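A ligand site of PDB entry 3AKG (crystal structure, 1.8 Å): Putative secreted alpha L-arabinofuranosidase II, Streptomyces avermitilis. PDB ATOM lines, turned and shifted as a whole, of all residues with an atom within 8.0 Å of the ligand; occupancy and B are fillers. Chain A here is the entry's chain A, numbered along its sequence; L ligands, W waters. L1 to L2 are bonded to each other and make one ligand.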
ATOM      1  N   ARG A 336     -30.314   6.901 -28.035  1.00  0.00           N
ATOM      2  CA  ARG A 336     -29.681   7.708 -26.995  1.00  0.00           C
ATOM      3  C   ARG A 336     -29.930   7.081 -25.621  1.00  0.00           C
ATOM      4  O   ARG A 336     -30.875   6.321 -25.458  1.00  0.00           O
ATOM      5  CB  ARG A 336     -30.184   9.164 -27.023  1.00  0.00           C
ATOM      6  CG  ARG A 336     -31.691   9.392 -26.630  1.00  0.00           C
ATOM      7  CD  ARG A 336     -31.907   9.613 -25.109  1.00  0.00           C
ATOM      8  NE  ARG A 336     -31.045  10.667 -24.545  1.00  0.00           N
ATOM      9  CZ  ARG A 336     -31.279  11.982 -24.638  1.00  0.00           C
ATOM     10  NH1 ARG A 336     -32.361  12.453 -25.282  1.00  0.00           N
ATOM     11  NH2 ARG A 336     -30.418  12.825 -24.087  1.00  0.00           N
ATOM     12  N   HIS A 337     -29.089   7.408 -24.646  1.00  0.00           N
ATOM     13  CA  HIS A 337     -29.379   6.963 -23.279  1.00  0.00           C
ATOM     14  C   HIS A 337     -29.862   8.110 -22.397  1.00  0.00           C
ATOM     15  O   HIS A 337     -29.451   9.258 -22.569  1.00  0.00           O
ATOM     16  CB  HIS A 337     -28.182   6.215 -22.656  1.00  0.00           C
ATOM     17  CG  HIS A 337     -26.913   7.006 -22.567  1.00  0.00           C
ATOM     18  ND1 HIS A 337     -26.578   7.761 -21.459  1.00  0.00           N
ATOM     19  CD2 HIS A 337     -25.875   7.132 -23.425  1.00  0.00           C
ATOM     20  CE1 HIS A 337     -25.400   8.330 -21.645  1.00  0.00           C
ATOM     21  NE2 HIS A 337     -24.951   7.972 -22.837  1.00  0.00           N
ATOM     22  N   TRP A 338     -30.762   7.776 -21.475  1.00  0.00           N
ATOM     23  CA  TRP A 338     -31.236   8.696 -20.436  1.00  0.00           C
ATOM     24  C   TRP A 338     -31.442   7.890 -19.140  1.00  0.00           C
ATOM     25  O   TRP A 338     -32.176   6.893 -19.154  1.00  0.00           O
ATOM     26  CB  TRP A 338     -32.560   9.383 -20.837  1.00  0.00           C
ATOM     27  CG  TRP A 338     -32.923  10.459 -19.869  1.00  0.00           C
ATOM     28  CD1 TRP A 338     -33.556  10.320 -18.649  1.00  0.00           C
ATOM     29  CD2 TRP A 338     -32.606  11.851 -20.004  1.00  0.00           C
ATOM     30  NE1 TRP A 338     -33.650  11.544 -18.029  1.00  0.00           N
ATOM     31  CE2 TRP A 338     -33.077  12.506 -18.836  1.00  0.00           C
ATOM     32  CE3 TRP A 338     -31.964  12.611 -20.986  1.00  0.00           C
ATOM     33  CZ2 TRP A 338     -32.935  13.877 -18.629  1.00  0.00           C
ATOM     34  CZ3 TRP A 338     -31.828  13.985 -20.800  1.00  0.00           C
ATOM     35  CH2 TRP A 338     -32.313  14.608 -19.624  1.00  0.00           C
ATOM     36  N   ASP A 339     -30.822   8.353 -18.049  1.00  0.00           N
ATOM     37  CA  ASP A 339     -30.686   7.557 -16.799  1.00  0.00           C
ATOM     38  C   ASP A 339     -30.138   6.167 -17.110  1.00  0.00           C
ATOM     39  O   ASP A 339     -30.560   5.166 -16.534  1.00  0.00           O
ATOM     40  CB  ASP A 339     -32.033   7.457 -16.046  1.00  0.00           C
ATOM     41  CG  ASP A 339     -32.483   8.784 -15.449  1.00  0.00           C
ATOM     42  OD1 ASP A 339     -31.618   9.567 -14.965  1.00  0.00           O
ATOM     43  OD2 ASP A 339     -33.715   9.056 -15.463  1.00  0.00           O
ATOM     44  N   PHE A 340     -29.245   6.127 -18.101  1.00  0.00           N
ATOM     45  CA  PHE A 340     -28.639   4.913 -18.610  1.00  0.00           C
ATOM     46  C   PHE A 340     -29.517   3.907 -19.346  1.00  0.00           C
ATOM     47  O   PHE A 340     -29.019   2.878 -19.772  1.00  0.00           O
ATOM     48  CB  PHE A 340     -27.736   4.257 -17.558  1.00  0.00           C
ATOM     49  CG  PHE A 340     -26.684   5.178 -17.067  1.00  0.00           C
ATOM     50  CD1 PHE A 340     -25.568   5.455 -17.841  1.00  0.00           C
ATOM     51  CD2 PHE A 340     -26.839   5.835 -15.839  1.00  0.00           C
ATOM     52  CE1 PHE A 340     -24.576   6.328 -17.382  1.00  0.00           C
ATOM     53  CE2 PHE A 340     -25.861   6.720 -15.392  1.00  0.00           C
ATOM     54  CZ  PHE A 340     -24.744   6.967 -16.171  1.00  0.00           C
ATOM     55  N   ARG A 341     -30.801   4.217 -19.542  1.00  0.00           N
ATOM     56  CA  ARG A 341     -31.696   3.362 -20.340  1.00  0.00           C
ATOM     57  C   ARG A 341     -31.678   3.794 -21.810  1.00  0.00           C
ATOM     58  O   ARG A 341     -31.783   4.988 -22.069  1.00  0.00           O
ATOM     59  CB  ARG A 341     -33.126   3.432 -19.777  1.00  0.00           C
ATOM     60  CG  ARG A 341     -34.121   2.521 -20.501  1.00  0.00           C
ATOM     61  CD  ARG A 341     -33.971   1.054 -20.112  1.00  0.00           C
ATOM     62  NE  ARG A 341     -35.135   0.274 -20.562  1.00  0.00           N
ATOM     63  CZ  ARG A 341     -35.253  -0.274 -21.766  1.00  0.00           C
ATOM     64  NH1 ARG A 341     -34.283  -0.163 -22.672  1.00  0.00           N
ATOM     65  NH2 ARG A 341     -36.347  -0.940 -22.087  1.00  0.00           N
ATOM     66  N   ALA A 342     -31.561   2.843 -22.736  1.00  0.00           N
ATOM     67  CA  ALA A 342     -31.470   3.162 -24.179  1.00  0.00           C
ATOM     68  C   ALA A 342     -32.845   3.279 -24.825  1.00  0.00           C
ATOM     69  O   ALA A 342     -33.743   2.467 -24.577  1.00  0.00           O
ATOM     70  CB  ALA A 342     -30.634   2.125 -24.911  1.00  0.00           C
ATOM     71  N   VAL A 348     -32.127  15.527 -29.733  1.00  0.00           N
ATOM     72  CA  VAL A 348     -31.281  15.237 -28.579  1.00  0.00           C
ATOM     73  C   VAL A 348     -30.394  16.455 -28.267  1.00  0.00           C
ATOM     74  O   VAL A 348     -29.470  16.765 -29.034  1.00  0.00           O
ATOM     75  CB  VAL A 348     -30.442  13.990 -28.829  1.00  0.00           C
ATOM     76  CG1 VAL A 348     -29.526  13.677 -27.634  1.00  0.00           C
ATOM     77  CG2 VAL A 348     -31.337  12.791 -29.131  1.00  0.00           C
ATOM     78  N   THR A 349     -30.679  17.127 -27.162  1.00  0.00           N
ATOM     79  CA  THR A 349     -29.952  18.332 -26.742  1.00  0.00           C
ATOM     80  C   THR A 349     -28.580  17.965 -26.180  1.00  0.00           C
ATOM     81  O   THR A 349     -27.576  18.608 -26.482  1.00  0.00           O
ATOM     82  CB  THR A 349     -30.734  19.046 -25.631  1.00  0.00           C
ATOM     83  OG1 THR A 349     -32.083  19.254 -26.083  1.00  0.00           O
ATOM     84  CG2 THR A 349     -30.086  20.367 -25.259  1.00  0.00           C
ATOM     85  N   ASN A 350     -28.558  16.935 -25.323  1.00  0.00           N
ATOM     86  CA  ASN A 350     -27.307  16.401 -24.820  1.00  0.00           C
ATOM     87  C   ASN A 350     -26.698  15.441 -25.826  1.00  0.00           C
ATOM     88  O   ASN A 350     -26.843  14.227 -25.692  1.00  0.00           O
ATOM     89  CB  ASN A 350     -27.498  15.748 -23.463  1.00  0.00           C
ATOM     90  CG  ASN A 350     -26.222  15.725 -22.669  1.00  0.00           C
ATOM     91  OD1 ASN A 350     -25.410  16.634 -22.782  1.00  0.00           O
ATOM     92  ND2 ASN A 350     -26.035  14.690 -21.872  1.00  0.00           N
ATOM     93  N   LEU A 351     -26.042  16.012 -26.831  1.00  0.00           N
ATOM     94  CA  LEU A 351     -25.660  15.289 -28.035  1.00  0.00           C
ATOM     95  C   LEU A 351     -24.922  13.964 -27.770  1.00  0.00           C
ATOM     96  O   LEU A 351     -25.201  12.966 -28.422  1.00  0.00           O
ATOM     97  CB  LEU A 351     -24.785  16.207 -28.940  1.00  0.00           C
ATOM     98  CG  LEU A 351     -24.309  15.543 -30.239  1.00  0.00           C
ATOM     99  CD1 LEU A 351     -25.506  15.267 -31.173  1.00  0.00           C
ATOM    100  CD2 LEU A 351     -23.263  16.436 -30.950  1.00  0.00           C
ATOM    101  N   ALA A 352     -23.992  13.966 -26.824  1.00  0.00           N
ATOM    102  CA  ALA A 352     -23.138  12.813 -26.593  1.00  0.00           C
ATOM    103  C   ALA A 352     -23.898  11.584 -26.057  1.00  0.00           C
ATOM    104  O   ALA A 352     -23.415  10.474 -26.174  1.00  0.00           O
ATOM    105  CB  ALA A 352     -21.956  13.174 -25.688  1.00  0.00           C
ATOM    106  N   ASP A 353     -25.085  11.805 -25.497  1.00  0.00           N
ATOM    107  CA  ASP A 353     -25.970  10.681 -25.135  1.00  0.00           C
ATOM    108  C   ASP A 353     -26.377   9.872 -26.362  1.00  0.00           C
ATOM    109  O   ASP A 353     -26.858   8.727 -26.219  1.00  0.00           O
ATOM    110  CB  ASP A 353     -27.261  11.180 -24.497  1.00  0.00           C
ATOM    111  CG  ASP A 353     -27.077  11.681 -23.112  1.00  0.00           C
ATOM    112  OD1 ASP A 353     -25.995  11.465 -22.477  1.00  0.00           O
ATOM    113  OD2 ASP A 353     -28.053  12.289 -22.634  1.00  0.00           O
ATOM    114  N   SER A 354     -26.190  10.448 -27.559  1.00  0.00           N
ATOM    115  CA  SER A 354     -26.630   9.801 -28.789  1.00  0.00           C
ATOM    116  C   SER A 354     -25.475   9.413 -29.700  1.00  0.00           C
ATOM    117  O   SER A 354     -25.680   9.107 -30.860  1.00  0.00           O
ATOM    118  CB  SER A 354     -27.692  10.652 -29.514  1.00  0.00           C
ATOM    119  OG  SER A 354     -27.127  11.838 -30.077  1.00  0.00           O
ATOM    120  N   SER A 372     -20.204   3.914 -25.522  1.00  0.00           N
ATOM    121  CA  SER A 372     -20.741   5.260 -25.311  1.00  0.00           C
ATOM    122  C   SER A 372     -19.650   6.346 -25.459  1.00  0.00           C
ATOM    123  O   SER A 372     -18.530   6.184 -24.964  1.00  0.00           O
ATOM    124  CB  SER A 372     -21.387   5.356 -23.924  1.00  0.00           C
ATOM    125  OG  SER A 372     -21.576   6.702 -23.516  1.00  0.00           O
ATOM    126  N   ASN A 374     -19.831   9.582 -24.261  1.00  0.00           N
ATOM    127  CA  ASN A 374     -19.664  10.352 -23.034  1.00  0.00           C
ATOM    128  C   ASN A 374     -19.364   9.512 -21.793  1.00  0.00           C
ATOM    129  O   ASN A 374     -18.992  10.057 -20.761  1.00  0.00           O
ATOM    130  CB  ASN A 374     -20.827  11.337 -22.800  1.00  0.00           C
ATOM    131  CG  ASN A 374     -22.221  10.686 -22.848  1.00  0.00           C
ATOM    132  OD1 ASN A 374     -22.387   9.517 -23.174  1.00  0.00           O
ATOM    133  ND2 ASN A 374     -23.234  11.489 -22.518  1.00  0.00           N
ATOM    134  N   TYR A 375     -19.532   8.187 -21.914  1.00  0.00           N
ATOM    135  CA  TYR A 375     -19.159   7.258 -20.851  1.00  0.00           C
ATOM    136  C   TYR A 375     -18.236   6.167 -21.424  1.00  0.00           C
ATOM    137  O   TYR A 375     -18.675   5.023 -21.653  1.00  0.00           O
ATOM    138  CB  TYR A 375     -20.410   6.651 -20.199  1.00  0.00           C
ATOM    139  CG  TYR A 375     -21.149   7.641 -19.343  1.00  0.00           C
ATOM    140  CD1 TYR A 375     -22.090   8.519 -19.901  1.00  0.00           C
ATOM    141  CD2 TYR A 375     -20.881   7.745 -17.991  1.00  0.00           C
ATOM    142  CE1 TYR A 375     -22.776   9.440 -19.105  1.00  0.00           C
ATOM    143  CE2 TYR A 375     -21.553   8.664 -17.181  1.00  0.00           C
ATOM    144  CZ  TYR A 375     -22.493   9.503 -17.746  1.00  0.00           C
ATOM    145  OH  TYR A 375     -23.142  10.406 -16.958  1.00  0.00           O
ATOM    146  N   TYR A 378     -18.292   2.220 -21.103  1.00  0.00           N
ATOM    147  CA  TYR A 378     -19.678   1.781 -20.952  1.00  0.00           C
ATOM    148  C   TYR A 378     -20.179   1.441 -22.334  1.00  0.00           C
ATOM    149  O   TYR A 378     -19.773   2.051 -23.319  1.00  0.00           O
ATOM    150  CB  TYR A 378     -20.607   2.880 -20.428  1.00  0.00           C
ATOM    151  CG  TYR A 378     -20.451   3.322 -18.996  1.00  0.00           C
ATOM    152  CD1 TYR A 378     -19.199   3.655 -18.466  1.00  0.00           C
ATOM    153  CD2 TYR A 378     -21.575   3.482 -18.172  1.00  0.00           C
ATOM    154  CE1 TYR A 378     -19.067   4.095 -17.150  1.00  0.00           C
ATOM    155  CE2 TYR A 378     -21.451   3.933 -16.862  1.00  0.00           C
ATOM    156  CZ  TYR A 378     -20.189   4.231 -16.359  1.00  0.00           C
ATOM    157  OH  TYR A 378     -20.057   4.685 -15.069  1.00  0.00           O
ATOM    158  N   TRP A 388     -29.543  -1.121 -21.976  1.00  0.00           N
ATOM    159  CA  TRP A 388     -29.039  -0.094 -21.076  1.00  0.00           C
ATOM    160  C   TRP A 388     -27.632   0.244 -21.537  1.00  0.00           C
ATOM    161  O   TRP A 388     -27.037  -0.501 -22.307  1.00  0.00           O
ATOM    162  CB  TRP A 388     -28.968  -0.607 -19.645  1.00  0.00           C
ATOM    163  CG  TRP A 388     -30.289  -0.957 -19.032  1.00  0.00           C
ATOM    164  CD1 TRP A 388     -31.012  -2.094 -19.240  1.00  0.00           C
ATOM    165  CD2 TRP A 388     -31.032  -0.174 -18.088  1.00  0.00           C
ATOM    166  NE1 TRP A 388     -32.179  -2.065 -18.489  1.00  0.00           N
ATOM    167  CE2 TRP A 388     -32.203  -0.895 -17.776  1.00  0.00           C
ATOM    168  CE3 TRP A 388     -30.821   1.075 -17.490  1.00  0.00           C
ATOM    169  CZ2 TRP A 388     -33.170  -0.406 -16.879  1.00  0.00           C
ATOM    170  CZ3 TRP A 388     -31.780   1.565 -16.601  1.00  0.00           C
ATOM    171  CH2 TRP A 388     -32.936   0.807 -16.308  1.00  0.00           C
ATOM    172  N   VAL A 389     -27.102   1.358 -21.038  1.00  0.00           N
ATOM    173  CA  VAL A 389     -25.703   1.707 -21.254  1.00  0.00           C
ATOM    174  C   VAL A 389     -25.009   1.524 -19.915  1.00  0.00           C
ATOM    175  O   VAL A 389     -25.311   2.219 -18.957  1.00  0.00           O
ATOM    176  CB  VAL A 389     -25.536   3.139 -21.796  1.00  0.00           C
ATOM    177  CG1 VAL A 389     -24.065   3.565 -21.725  1.00  0.00           C
ATOM    178  CG2 VAL A 389     -26.048   3.221 -23.224  1.00  0.00           C
HETATM  179  O1  LIG L   1     -29.163  12.781 -17.046  1.00  0.00           O
HETATM  180  C1  LIG L   1     -30.012  12.249 -16.019  1.00  0.00           C
HETATM  181  C2  LIG L   1     -30.644  13.438 -15.363  1.00  0.00           C
HETATM  182  O2  LIG L   1     -29.689  14.101 -14.495  1.00  0.00           O
HETATM  183  C3  LIG L   1     -31.717  12.950 -14.407  1.00  0.00           C
HETATM  184  O3  LIG L   1     -32.922  12.635 -15.105  1.00  0.00           O
HETATM  185  C4  LIG L   1     -31.947  14.217 -13.583  1.00  0.00           C
HETATM  186  O4  LIG L   1     -32.442  13.858 -12.288  1.00  0.00           O
HETATM  187  C5  LIG L   1     -30.524  14.812 -13.500  1.00  0.00           C
HETATM  188  O5  LIG L   1     -30.626  16.216 -13.804  1.00  0.00           O
HETATM  189  O1  LG2 L   2     -28.049   8.239 -19.296  1.00  0.00           O
HETATM  190  C1  LG2 L   2     -27.247   8.830 -18.265  1.00  0.00           C
HETATM  191  C2  LG2 L   2     -27.430  10.361 -18.185  1.00  0.00           C
HETATM  192  O2  LG2 L   2     -28.790  10.587 -17.752  1.00  0.00           O
HETATM  193  C3  LG2 L   2     -27.342  11.108 -19.515  1.00  0.00           C
HETATM  194  O3  LG2 L   2     -25.957  11.374 -19.853  1.00  0.00           O
HETATM  195  C4  LG2 L   2     -28.039  12.417 -19.114  1.00  0.00           C
HETATM  196  O4  LG2 L   2     -28.565  13.143 -20.266  1.00  0.00           O
HETATM  197  C5  LG2 L   2     -29.161  11.924 -18.197  1.00  0.00           C
HETATM  198  O   HOH W   1     -24.270  12.472 -18.253  1.00  0.00           O
HETATM  199  O   HOH W   2     -29.049  15.796 -19.854  1.00  0.00           O
HETATM  200  O   HOH W   3     -34.586  11.012 -13.901  1.00  0.00           O
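Water W1 bridges an oxygen (O3) of LG2 L2 (2.6 Å) and the side-chain hydroxyl (OH) of Tyr 375 (2.7 Å).
Water W3 bridges O3 of LIG L1 and OD2 of Asp 339.
A ring nitrogen (ND1) of His 337 sits at hydrogen-bond distance from an oxygen (O1) of LG2 L2 (2.7 Å).
An oxygen (O1) of LG2 L2 sits at hydrogen-bond distance from the backbone NH (N) of Phe 340, 2.7 Å away.
The side-chain carboxylate of Asp 339 lies close to an oxygen (O3) of LIG L1, 3.3 Å away.
The indole nitrogen (NE1) of Trp 338 is in hydrogen-bond range of an oxygen (O3) of LIG L1 (3.2 Å).
O2 of LG2 L2 is in hydrogen-bond range of N of Asp 339, at 3.0 Å.
The side-chain carboxylate (OD2) of Asp 353 lies within hydrogen-bond range of an oxygen (O4) of LG2 L2 (2.6 Å).
ND2 of Asn 350 lies within hydrogen-bond range of O4 of LG2 L2, at 3.4 Å.
OD1 of Asn 374 sits at hydrogen-bond distance from OG of Ser 372, at 2.9 Å.
The backbone carbonyl oxygen (O) of Phe 340 is in hydrogen-bond range of the backbone NH (N) of Val 389 (2.8 Å).
OD1 of Asn 374 is in hydrogen-bond range of NE2 of His 337.
The side-chain amide nitrogen (ND2) of Asn 374 lies within hydrogen-bond range of the side-chain carboxylate (OD1) of Asp 353 (2.8 Å).
The backbone carbonyl oxygen (O) of Asp 353 is in hydrogen-bond range of the backbone NH (N) of His 337.
The guanidinium group (NH2) of Arg 336 lies within salt-bridge range of the side-chain carboxylate (OD2) of Asp 353 (2.8 Å).
The side-chain hydroxyl of Ser 372 lies within hydrogen-bond range of the backbone NH of Tyr 375, 3.0 Å away.
OD1 of Asn 374 lies close to O of Ala 352 (3.3 Å).
Asn 374 touches the ligand.
Tyr 375 touches the ligand.
The nearest printed residue that does not touch the ligand is Arg 336 (4.3 Å).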
